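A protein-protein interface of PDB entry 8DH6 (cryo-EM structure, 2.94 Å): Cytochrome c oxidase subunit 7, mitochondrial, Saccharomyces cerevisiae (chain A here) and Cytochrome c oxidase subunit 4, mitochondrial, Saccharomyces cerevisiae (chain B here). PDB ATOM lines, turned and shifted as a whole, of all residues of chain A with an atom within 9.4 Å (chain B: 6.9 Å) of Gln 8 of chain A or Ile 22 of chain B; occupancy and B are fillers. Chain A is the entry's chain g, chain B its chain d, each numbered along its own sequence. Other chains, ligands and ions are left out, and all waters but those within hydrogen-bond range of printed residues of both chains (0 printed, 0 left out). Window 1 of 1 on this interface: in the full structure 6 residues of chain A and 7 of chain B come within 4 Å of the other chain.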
ATOM      1  N   ASN A   2      28.866   4.871  14.215  1.00  0.00           N
ATOM      2  CA  ASN A   2      28.959   3.589  13.514  1.00  0.00           C
ATOM      3  C   ASN A   2      28.487   2.434  14.400  1.00  0.00           C
ATOM      4  O   ASN A   2      29.253   1.555  14.794  1.00  0.00           O
ATOM      5  CB  ASN A   2      30.382   3.346  13.004  1.00  0.00           C
ATOM      6  CG  ASN A   2      30.456   2.195  12.027  1.00  0.00           C
ATOM      7  OD1 ASN A   2      29.432   1.702  11.554  1.00  0.00           O
ATOM      8  ND2 ASN A   2      31.670   1.755  11.722  1.00  0.00           N
ATOM      9  N   LYS A   3      27.194   2.460  14.718  1.00  0.00           N
ATOM     10  CA  LYS A   3      26.549   1.388  15.459  1.00  0.00           C
ATOM     11  C   LYS A   3      25.708   0.484  14.565  1.00  0.00           C
ATOM     12  O   LYS A   3      24.902  -0.301  15.075  1.00  0.00           O
ATOM     13  CB  LYS A   3      25.684   1.971  16.576  1.00  0.00           C
ATOM     14  CG  LYS A   3      26.463   2.767  17.607  1.00  0.00           C
ATOM     15  CD  LYS A   3      27.379   1.868  18.421  1.00  0.00           C
ATOM     16  CE  LYS A   3      27.702   2.487  19.772  1.00  0.00           C
ATOM     17  NZ  LYS A   3      28.611   1.623  20.574  1.00  0.00           N
ATOM     18  N   VAL A   4      25.882   0.573  13.244  1.00  0.00           N
ATOM     19  CA  VAL A   4      24.960  -0.087  12.324  1.00  0.00           C
ATOM     20  C   VAL A   4      25.070  -1.604  12.428  1.00  0.00           C
ATOM     21  O   VAL A   4      24.057  -2.308  12.409  1.00  0.00           O
ATOM     22  CB  VAL A   4      25.201   0.405  10.888  1.00  0.00           C
ATOM     23  CG1 VAL A   4      24.181  -0.206   9.945  1.00  0.00           C
ATOM     24  CG2 VAL A   4      25.134   1.918  10.838  1.00  0.00           C
ATOM     25  N   ILE A   5      26.289  -2.135  12.529  1.00  0.00           N
ATOM     26  CA  ILE A   5      26.459  -3.586  12.595  1.00  0.00           C
ATOM     27  C   ILE A   5      25.936  -4.133  13.919  1.00  0.00           C
ATOM     28  O   ILE A   5      25.275  -5.180  13.961  1.00  0.00           O
ATOM     29  CB  ILE A   5      27.935  -3.957  12.369  1.00  0.00           C
ATOM     30  CG1 ILE A   5      28.382  -3.498  10.984  1.00  0.00           C
ATOM     31  CG2 ILE A   5      28.144  -5.448  12.524  1.00  0.00           C
ATOM     32  CD1 ILE A   5      27.603  -4.135   9.863  1.00  0.00           C
ATOM     33  N   GLN A   6      26.230  -3.441  15.021  1.00  0.00           N
ATOM     34  CA  GLN A   6      25.735  -3.867  16.323  1.00  0.00           C
ATOM     35  C   GLN A   6      24.213  -3.872  16.358  1.00  0.00           C
ATOM     36  O   GLN A   6      23.593  -4.831  16.837  1.00  0.00           O
ATOM     37  CB  GLN A   6      26.298  -2.950  17.407  1.00  0.00           C
ATOM     38  CG  GLN A   6      25.751  -3.198  18.792  1.00  0.00           C
ATOM     39  CD  GLN A   6      26.137  -2.099  19.759  1.00  0.00           C
ATOM     40  OE1 GLN A   6      26.920  -1.210  19.425  1.00  0.00           O
ATOM     41  NE2 GLN A   6      25.590  -2.155  20.969  1.00  0.00           N
ATOM     42  N   LEU A   7      23.590  -2.815  15.838  1.00  0.00           N
ATOM     43  CA  LEU A   7      22.135  -2.771  15.801  1.00  0.00           C
ATOM     44  C   LEU A   7      21.560  -3.778  14.814  1.00  0.00           C
ATOM     45  O   LEU A   7      20.448  -4.265  15.021  1.00  0.00           O
ATOM     46  CB  LEU A   7      21.648  -1.359  15.482  1.00  0.00           C
ATOM     47  CG  LEU A   7      21.496  -0.370  16.641  1.00  0.00           C
ATOM     48  CD1 LEU A   7      20.422  -0.868  17.588  1.00  0.00           C
ATOM     49  CD2 LEU A   7      22.792  -0.142  17.392  1.00  0.00           C
ATOM     50  N   GLN A   8      22.289  -4.109  13.747  1.00  0.00           N
ATOM     51  CA  GLN A   8      21.840  -5.177  12.858  1.00  0.00           C
ATOM     52  C   GLN A   8      21.802  -6.510  13.593  1.00  0.00           C
ATOM     53  O   GLN A   8      20.835  -7.273  13.466  1.00  0.00           O
ATOM     54  CB  GLN A   8      22.751  -5.270  11.633  1.00  0.00           C
ATOM     55  CG  GLN A   8      22.404  -4.297  10.521  1.00  0.00           C
ATOM     56  CD  GLN A   8      23.427  -4.289   9.405  1.00  0.00           C
ATOM     57  OE1 GLN A   8      24.375  -5.069   9.411  1.00  0.00           O
ATOM     58  NE2 GLN A   8      23.238  -3.402   8.438  1.00  0.00           N
ATOM     59  N   LYS A   9      22.844  -6.794  14.374  1.00  0.00           N
ATOM     60  CA  LYS A   9      22.850  -8.007  15.186  1.00  0.00           C
ATOM     61  C   LYS A   9      21.703  -8.004  16.187  1.00  0.00           C
ATOM     62  O   LYS A   9      21.039  -9.028  16.380  1.00  0.00           O
ATOM     63  CB  LYS A   9      24.186  -8.148  15.913  1.00  0.00           C
ATOM     64  CG  LYS A   9      25.379  -8.384  15.010  1.00  0.00           C
ATOM     65  CD  LYS A   9      26.647  -8.517  15.833  1.00  0.00           C
ATOM     66  CE  LYS A   9      27.871  -8.717  14.963  1.00  0.00           C
ATOM     67  NZ  LYS A   9      29.100  -8.834  15.793  1.00  0.00           N
ATOM     68  N   ILE A  10      21.460  -6.863  16.835  1.00  0.00           N
ATOM     69  CA  ILE A  10      20.385  -6.780  17.822  1.00  0.00           C
ATOM     70  C   ILE A  10      19.024  -6.974  17.162  1.00  0.00           C
ATOM     71  O   ILE A  10      18.159  -7.683  17.689  1.00  0.00           O
ATOM     72  CB  ILE A  10      20.457  -5.443  18.578  1.00  0.00           C
ATOM     73  CG1 ILE A  10      21.763  -5.344  19.367  1.00  0.00           C
ATOM     74  CG2 ILE A  10      19.270  -5.293  19.509  1.00  0.00           C
ATOM     75  CD1 ILE A  10      22.024  -3.969  19.924  1.00  0.00           C
ATOM     76  N   PHE A  11      18.809  -6.349  16.004  1.00  0.00           N
ATOM     77  CA  PHE A  11      17.515  -6.363  15.341  1.00  0.00           C
ATOM     78  C   PHE A  11      17.196  -7.696  14.684  1.00  0.00           C
ATOM     79  O   PHE A  11      16.027  -8.095  14.666  1.00  0.00           O
ATOM     80  CB  PHE A  11      17.463  -5.259  14.284  1.00  0.00           C
ATOM     81  CG  PHE A  11      16.827  -3.990  14.764  1.00  0.00           C
ATOM     82  CD1 PHE A  11      17.531  -3.110  15.563  1.00  0.00           C
ATOM     83  CD2 PHE A  11      15.526  -3.679  14.416  1.00  0.00           C
ATOM     84  CE1 PHE A  11      16.952  -1.943  16.006  1.00  0.00           C
ATOM     85  CE2 PHE A  11      14.941  -2.514  14.856  1.00  0.00           C
ATOM     86  CZ  PHE A  11      15.654  -1.645  15.652  1.00  0.00           C
ATOM     87  N   GLN A  12      18.194  -8.390  14.141  1.00  0.00           N
ATOM     88  CA  GLN A  12      17.939  -9.647  13.455  1.00  0.00           C
ATOM     89  C   GLN A  12      17.794 -10.831  14.400  1.00  0.00           C
ATOM     90  O   GLN A  12      17.349 -11.898  13.964  1.00  0.00           O
ATOM     91  CB  GLN A  12      19.053  -9.929  12.443  1.00  0.00           C
ATOM     92  CG  GLN A  12      19.041  -8.972  11.269  1.00  0.00           C
ATOM     93  CD  GLN A  12      20.044  -9.342  10.204  1.00  0.00           C
ATOM     94  OE1 GLN A  12      20.380 -10.512  10.033  1.00  0.00           O
ATOM     95  NE2 GLN A  12      20.527  -8.346   9.479  1.00  0.00           N
ATOM     96  N   SER A  13      18.150 -10.672  15.672  1.00  0.00           N
ATOM     97  CA  SER A  13      17.963 -11.709  16.683  1.00  0.00           C
ATOM     98  C   SER A  13      17.151 -11.104  17.824  1.00  0.00           C
ATOM     99  O   SER A  13      17.697 -10.635  18.823  1.00  0.00           O
ATOM    100  CB  SER A  13      19.304 -12.241  17.169  1.00  0.00           C
ATOM    101  OG  SER A  13      19.999 -11.254  17.911  1.00  0.00           O
ATOM    102  N   SER A  14      15.828 -11.123  17.670  1.00  0.00           N
ATOM    103  CA  SER A  14      14.928 -10.583  18.682  1.00  0.00           C
ATOM    104  C   SER A  14      13.511 -11.101  18.482  1.00  0.00           C
ATOM    105  O   SER A  14      12.925 -10.929  17.409  1.00  0.00           O
ATOM    106  CB  SER A  14      14.932  -9.053  18.653  1.00  0.00           C
ATOM    107  OG  SER A  14      16.203  -8.532  18.995  1.00  0.00           O
ATOM    108  N   ARG A  21      12.290  -3.457  19.392  1.00  0.00           N
ATOM    109  CA  ARG A  21      13.581  -4.134  19.370  1.00  0.00           C
ATOM    110  C   ARG A  21      14.717  -3.250  19.867  1.00  0.00           C
ATOM    111  O   ARG A  21      15.650  -3.755  20.501  1.00  0.00           O
ATOM    112  CB  ARG A  21      13.883  -4.636  17.959  1.00  0.00           C
ATOM    113  CG  ARG A  21      13.279  -5.994  17.663  1.00  0.00           C
ATOM    114  CD  ARG A  21      13.606  -6.450  16.257  1.00  0.00           C
ATOM    115  NE  ARG A  21      12.762  -7.559  15.834  1.00  0.00           N
ATOM    116  CZ  ARG A  21      12.634  -7.965  14.580  1.00  0.00           C
ATOM    117  NH1 ARG A  21      13.283  -7.371  13.592  1.00  0.00           N
ATOM    118  NH2 ARG A  21      11.842  -8.997  14.310  1.00  0.00           N
ATOM    119  N   HIS A  22      14.669  -1.950  19.589  1.00  0.00           N
ATOM    120  CA  HIS A  22      15.718  -1.060  20.057  1.00  0.00           C
ATOM    121  C   HIS A  22      15.681  -0.957  21.581  1.00  0.00           C
ATOM    122  O   HIS A  22      14.605  -0.956  22.185  1.00  0.00           O
ATOM    123  CB  HIS A  22      15.564   0.327  19.441  1.00  0.00           C
ATOM    124  CG  HIS A  22      16.854   1.074  19.310  1.00  0.00           C
ATOM    125  ND1 HIS A  22      17.393   1.817  20.337  1.00  0.00           N
ATOM    126  CD2 HIS A  22      17.713   1.192  18.271  1.00  0.00           C
ATOM    127  CE1 HIS A  22      18.530   2.359  19.938  1.00  0.00           C
ATOM    128  NE2 HIS A  22      18.746   1.996  18.686  1.00  0.00           N
ATOM    129  N   LYS B   7      31.445 -16.585  10.083  1.00  0.00           N
ATOM    130  CA  LYS B   7      32.115 -15.698   9.146  1.00  0.00           C
ATOM    131  C   LYS B   7      31.094 -14.737   8.538  1.00  0.00           C
ATOM    132  O   LYS B   7      29.948 -14.649   8.985  1.00  0.00           O
ATOM    133  CB  LYS B   7      32.843 -16.515   8.080  1.00  0.00           C
ATOM    134  CG  LYS B   7      34.114 -17.188   8.572  1.00  0.00           C
ATOM    135  CD  LYS B   7      35.036 -16.198   9.261  1.00  0.00           C
ATOM    136  CE  LYS B   7      36.370 -16.835   9.613  1.00  0.00           C
ATOM    137  NZ  LYS B   7      36.195 -18.143  10.304  1.00  0.00           N
ATOM    138  N   THR B   8      31.502 -13.997   7.506  1.00  0.00           N
ATOM    139  CA  THR B   8      30.647 -12.986   6.894  1.00  0.00           C
ATOM    140  C   THR B   8      30.211 -13.366   5.483  1.00  0.00           C
ATOM    141  O   THR B   8      29.703 -12.510   4.750  1.00  0.00           O
ATOM    142  CB  THR B   8      31.349 -11.628   6.875  1.00  0.00           C
ATOM    143  OG1 THR B   8      32.559 -11.723   6.114  1.00  0.00           O
ATOM    144  CG2 THR B   8      31.679 -11.182   8.289  1.00  0.00           C
ATOM    145  N   ALA B   9      30.397 -14.627   5.086  1.00  0.00           N
ATOM    146  CA  ALA B   9      29.942 -15.134   3.789  1.00  0.00           C
ATOM    147  C   ALA B   9      30.556 -14.325   2.640  1.00  0.00           C
ATOM    148  O   ALA B   9      29.877 -13.598   1.914  1.00  0.00           O
ATOM    149  CB  ALA B   9      28.412 -15.137   3.713  1.00  0.00           C
ATOM    150  N   PRO B  18      20.637 -16.756   7.613  1.00  0.00           N
ATOM    151  CA  PRO B  18      20.589 -15.288   7.615  1.00  0.00           C
ATOM    152  C   PRO B  18      21.525 -14.622   8.608  1.00  0.00           C
ATOM    153  O   PRO B  18      21.677 -13.394   8.551  1.00  0.00           O
ATOM    154  CB  PRO B  18      19.125 -14.995   7.988  1.00  0.00           C
ATOM    155  CG  PRO B  18      18.382 -16.244   7.659  1.00  0.00           C
ATOM    156  CD  PRO B  18      19.338 -17.349   7.968  1.00  0.00           C
ATOM    157  N   GLU B  19      22.145 -15.376   9.516  1.00  0.00           N
ATOM    158  CA  GLU B  19      22.998 -14.778  10.534  1.00  0.00           C
ATOM    159  C   GLU B  19      24.433 -14.581  10.070  1.00  0.00           C
ATOM    160  O   GLU B  19      25.220 -13.965  10.796  1.00  0.00           O
ATOM    161  CB  GLU B  19      22.986 -15.633  11.803  1.00  0.00           C
ATOM    162  CG  GLU B  19      23.600 -17.009  11.631  1.00  0.00           C
ATOM    163  CD  GLU B  19      23.511 -17.849  12.889  1.00  0.00           C
ATOM    164  OE1 GLU B  19      22.947 -17.362  13.893  1.00  0.00           O
ATOM    165  OE2 GLU B  19      24.005 -18.996  12.876  1.00  0.00           O
ATOM    166  N   THR B  20      24.794 -15.085   8.894  1.00  0.00           N
ATOM    167  CA  THR B  20      26.132 -14.922   8.349  1.00  0.00           C
ATOM    168  C   THR B  20      26.194 -13.843   7.275  1.00  0.00           C
ATOM    169  O   THR B  20      27.205 -13.736   6.574  1.00  0.00           O
ATOM    170  CB  THR B  20      26.639 -16.250   7.786  1.00  0.00           C
ATOM    171  OG1 THR B  20      28.023 -16.128   7.441  1.00  0.00           O
ATOM    172  CG2 THR B  20      25.850 -16.632   6.552  1.00  0.00           C
ATOM    173  N   LEU B  21      25.138 -13.042   7.135  1.00  0.00           N
ATOM    174  CA  LEU B  21      25.043 -12.021   6.100  1.00  0.00           C
ATOM    175  C   LEU B  21      25.113 -10.608   6.668  1.00  0.00           C
ATOM    176  O   LEU B  21      24.373  -9.728   6.221  1.00  0.00           O
ATOM    177  CB  LEU B  21      23.750 -12.199   5.305  1.00  0.00           C
ATOM    178  CG  LEU B  21      23.673 -13.375   4.334  1.00  0.00           C
ATOM    179  CD1 LEU B  21      22.266 -13.517   3.788  1.00  0.00           C
ATOM    180  CD2 LEU B  21      24.665 -13.201   3.208  1.00  0.00           C
ATOM    181  N   ILE B  22      25.982 -10.368   7.649  1.00  0.00           N
ATOM    182  CA  ILE B  22      26.035  -9.064   8.303  1.00  0.00           C
ATOM    183  C   ILE B  22      27.275  -8.292   7.867  1.00  0.00           C
ATOM    184  O   ILE B  22      27.166  -7.206   7.285  1.00  0.00           O
ATOM    185  CB  ILE B  22      25.976  -9.222   9.832  1.00  0.00           C
ATOM    186  CG1 ILE B  22      24.567  -9.646  10.251  1.00  0.00           C
ATOM    187  CG2 ILE B  22      26.367  -7.928  10.519  1.00  0.00           C
ATOM    188  CD1 ILE B  22      24.362  -9.717  11.740  1.00  0.00           C
ATOM    189  N   GLY B  23      28.458  -8.832   8.146  1.00  0.00           N
ATOM    190  CA  GLY B  23      29.689  -8.225   7.697  1.00  0.00           C
ATOM    191  C   GLY B  23      30.173  -7.097   8.586  1.00  0.00           C
ATOM    192  O   GLY B  23      29.493  -6.678   9.525  1.00  0.00           O
ATOM    193  N   PRO B  24      31.378  -6.592   8.311  1.00  0.00           N
ATOM    194  CA  PRO B  24      31.917  -5.470   9.085  1.00  0.00           C
ATOM    195  C   PRO B  24      31.630  -4.124   8.437  1.00  0.00           C
ATOM    196  O   PRO B  24      31.626  -3.977   7.213  1.00  0.00           O
ATOM    197  CB  PRO B  24      33.422  -5.764   9.090  1.00  0.00           C
ATOM    198  CG  PRO B  24      33.658  -6.432   7.766  1.00  0.00           C
ATOM    199  CD  PRO B  24      32.367  -7.118   7.354  1.00  0.00           C
ATOM    200  N   GLY B  25      31.404  -3.121   9.279  1.00  0.00           N
ATOM    201  CA  GLY B  25      31.046  -1.803   8.804  1.00  0.00           C
ATOM    202  C   GLY B  25      32.250  -0.975   8.388  1.00  0.00           C
ATOM    203  O   GLY B  25      33.374  -1.458   8.249  1.00  0.00           O
ATOM    204  N   LEU B  35      29.315  -3.578   0.265  1.00  0.00           N
ATOM    205  CA  LEU B  35      29.818  -4.824   0.828  1.00  0.00           C
ATOM    206  C   LEU B  35      30.065  -4.729   2.327  1.00  0.00           C
ATOM    207  O   LEU B  35      30.302  -5.758   2.966  1.00  0.00           O
ATOM    208  CB  LEU B  35      31.106  -5.249   0.120  1.00  0.00           C
ATOM    209  CG  LEU B  35      30.986  -6.038  -1.187  1.00  0.00           C
ATOM    210  CD1 LEU B  35      30.312  -7.376  -0.926  1.00  0.00           C
ATOM    211  CD2 LEU B  35      30.255  -5.260  -2.276  1.00  0.00           C
ATOM    212  N   ASP B  36      30.025  -3.526   2.899  1.00  0.00           N
ATOM    213  CA  ASP B  36      30.327  -3.367   4.318  1.00  0.00           C
ATOM    214  C   ASP B  36      29.107  -3.629   5.193  1.00  0.00           C
ATOM    215  O   ASP B  36      29.150  -4.464   6.102  1.00  0.00           O
ATOM    216  CB  ASP B  36      30.882  -1.966   4.585  1.00  0.00           C
ATOM    217  CG  ASP B  36      32.381  -1.880   4.376  1.00  0.00           C
ATOM    218  OD1 ASP B  36      33.130  -2.398   5.230  1.00  0.00           O
ATOM    219  OD2 ASP B  36      32.813  -1.288   3.367  1.00  0.00           O
ATOM    220  N   GLN B  37      28.003  -2.927   4.936  1.00  0.00           N
ATOM    221  CA  GLN B  37      26.896  -2.893   5.883  1.00  0.00           C
ATOM    222  C   GLN B  37      25.576  -3.406   5.321  1.00  0.00           C
ATOM    223  O   GLN B  37      24.560  -3.347   6.022  1.00  0.00           O
ATOM    224  CB  GLN B  37      26.717  -1.470   6.416  1.00  0.00           C
ATOM    225  CG  GLN B  37      27.899  -0.985   7.228  1.00  0.00           C
ATOM    226  CD  GLN B  37      27.594   0.269   8.005  1.00  0.00           C
ATOM    227  OE1 GLN B  37      26.517   0.846   7.873  1.00  0.00           O
ATOM    228  NE2 GLN B  37      28.543   0.700   8.826  1.00  0.00           N
ATOM    229  N   GLU B  38      25.548  -3.902   4.088  1.00  0.00           N
ATOM    230  CA  GLU B  38      24.339  -4.547   3.595  1.00  0.00           C
ATOM    231  C   GLU B  38      24.115  -5.856   4.339  1.00  0.00           C
ATOM    232  O   GLU B  38      25.063  -6.582   4.648  1.00  0.00           O
ATOM    233  CB  GLU B  38      24.429  -4.804   2.093  1.00  0.00           C
ATOM    234  CG  GLU B  38      24.088  -3.602   1.230  1.00  0.00           C
ATOM    235  CD  GLU B  38      22.761  -2.971   1.599  1.00  0.00           C
ATOM    236  OE1 GLU B  38      21.776  -3.714   1.792  1.00  0.00           O
ATOM    237  OE2 GLU B  38      22.702  -1.727   1.695  1.00  0.00           O
ATOM    238  N   THR B  39      22.854  -6.157   4.633  1.00  0.00           N
ATOM    239  CA  THR B  39      22.511  -7.328   5.424  1.00  0.00           C
ATOM    240  C   THR B  39      21.257  -7.991   4.873  1.00  0.00           C
ATOM    241  O   THR B  39      20.458  -7.378   4.161  1.00  0.00           O
ATOM    242  CB  THR B  39      22.316  -6.964   6.901  1.00  0.00           C
ATOM    243  OG1 THR B  39      22.097  -8.156   7.662  1.00  0.00           O
ATOM    244  CG2 THR B  39      21.133  -6.037   7.066  1.00  0.00           C
ATOM    245  N   GLY B  40      21.106  -9.272   5.201  1.00  0.00           N
ATOM    246  CA  GLY B  40      19.883  -9.986   4.874  1.00  0.00           C
ATOM    247  C   GLY B  40      19.698 -10.200   3.384  1.00  0.00           C
ATOM    248  O   GLY B  40      20.643 -10.488   2.641  1.00  0.00           O
ATOM    249  N   ARG B  43      21.750  -8.039   1.045  1.00  0.00           N
ATOM    250  CA  ARG B  43      23.128  -8.520   0.975  1.00  0.00           C
ATOM    251  C   ARG B  43      23.235  -9.763   0.103  1.00  0.00           C
ATOM    252  O   ARG B  43      24.191  -9.909  -0.667  1.00  0.00           O
ATOM    253  CB  ARG B  43      23.649  -8.811   2.380  1.00  0.00           C
ATOM    254  CG  ARG B  43      25.058  -9.360   2.427  1.00  0.00           C
ATOM    255  CD  ARG B  43      26.061  -8.328   1.968  1.00  0.00           C
ATOM    256  NE  ARG B  43      27.421  -8.692   2.343  1.00  0.00           N
ATOM    257  CZ  ARG B  43      27.994  -8.360   3.490  1.00  0.00           C
ATOM    258  NH1 ARG B  43      27.348  -7.663   4.409  1.00  0.00           N
ATOM    259  NH2 ARG B  43      29.247  -8.738   3.722  1.00  0.00           N
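Among the printed residues, pairs that only touch across the chains: Ile 5 of chain A with Gly 23 of chain B (3.2 Å), Val 4 of chain A with Gln 37 of chain B (3.3 Å), Ile 5 of chain A with Gly 25 of chain B (3.5 Å), Gln 8 of chain A with Thr 39 of chain B (3.6 Å), Ile 5 of chain A with Ile 22 of chain B (3.7 Å), Gln 8 of chain A with Ile 22 of chain B (3.7 Å) and Lys 9 of chain A with Ile 22 of chain B (3.7 Å).
The backbone carbonyl oxygen (O) of Pro 18 of chain B lies close to the side-chain amide oxygen (OE1) of Gln 12 of chain A, 3.5 Å away.
The backbone carbonyl oxygen of Gln 37 of chain B sits at hydrogen-bond distance from the side-chain amide nitrogen of Gln 8 of chain A (2.8 Å).
OD1 of Asn 2 of chain A lies within hydrogen-bond range of NE2 of Gln 37 of chain B, 3.0 Å away.
NE2 of Gln 12 of chain A lies within hydrogen-bond range of OG1 of Thr 39 of chain B, 2.4 Å away.
Hydrophobic or aromatic side chains of chain B that line the printed part of chain A: Ile 22.
Printed residues of chain A that touch a printed residue of chain B: Asn 2, Val 4, Ile 5, Gln 8, Lys 9 and Gln 12.
Hydrophobic or aromatic side chains of chain A within 4 Å of the printed part of chain B: Val 4 and Ile 5.
Among the printed residues, 11 pairs touch across the chains.
Among the printed residues, no Asp or Glu carboxylate lies within 4 Å of a Lys or Arg side-chain nitrogen of the other chain.
Gln 8 of chain A touches three residues of chain B.
Of chain A, only Ile 5, Gln 8 and Lys 9 come within 4 Å of Ile 22 of chain B.
Of chain A, only Ile 5 comes within 4 Å of Gly 23 of chain B.
Of the printed residues of chain B, Lys 9 of chain A touches Ile 22.
Printed residues of chain A within 4 Å of Thr 39 of chain B: Gln 8 and Gln 12.
Printed residues of chain A within 4 Å of Gly 25 of chain B: Ile 5 (3.5 Å).
Of the printed residues of chain B, Ile 5 of chain A touches Ile 22 (3.7 Å), Gly 23 (3.2 Å) and Gly 25 (3.5 Å).
Pro 24 of chain B touches none of the printed residues of chain A.
Ala 9 of chain B touches none of the printed residues of chain A.
The nearest residue of chain A that does not touch Ile 22 of chain B is Gln 12 of chain A (4.3 Å).
The nearest printed residue of chain A that does not touch Thr 39 of chain B is Ile 5 of chain A (6.7 Å).
The guanidinium group of Arg 43 of chain B lies within hydrogen-bond range of the backbone carbonyl oxygen of Ile 22 of chain B, 2.9 Å away.
The backbone carbonyl oxygen of Leu 21 of chain B sits at hydrogen-bond distance from the side-chain hydroxyl of Thr 39 of chain B, at 3.1 Å.
O of Lys 9 of chain A is in hydrogen-bond range of OG of Ser 13 of chain A (2.9 Å).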
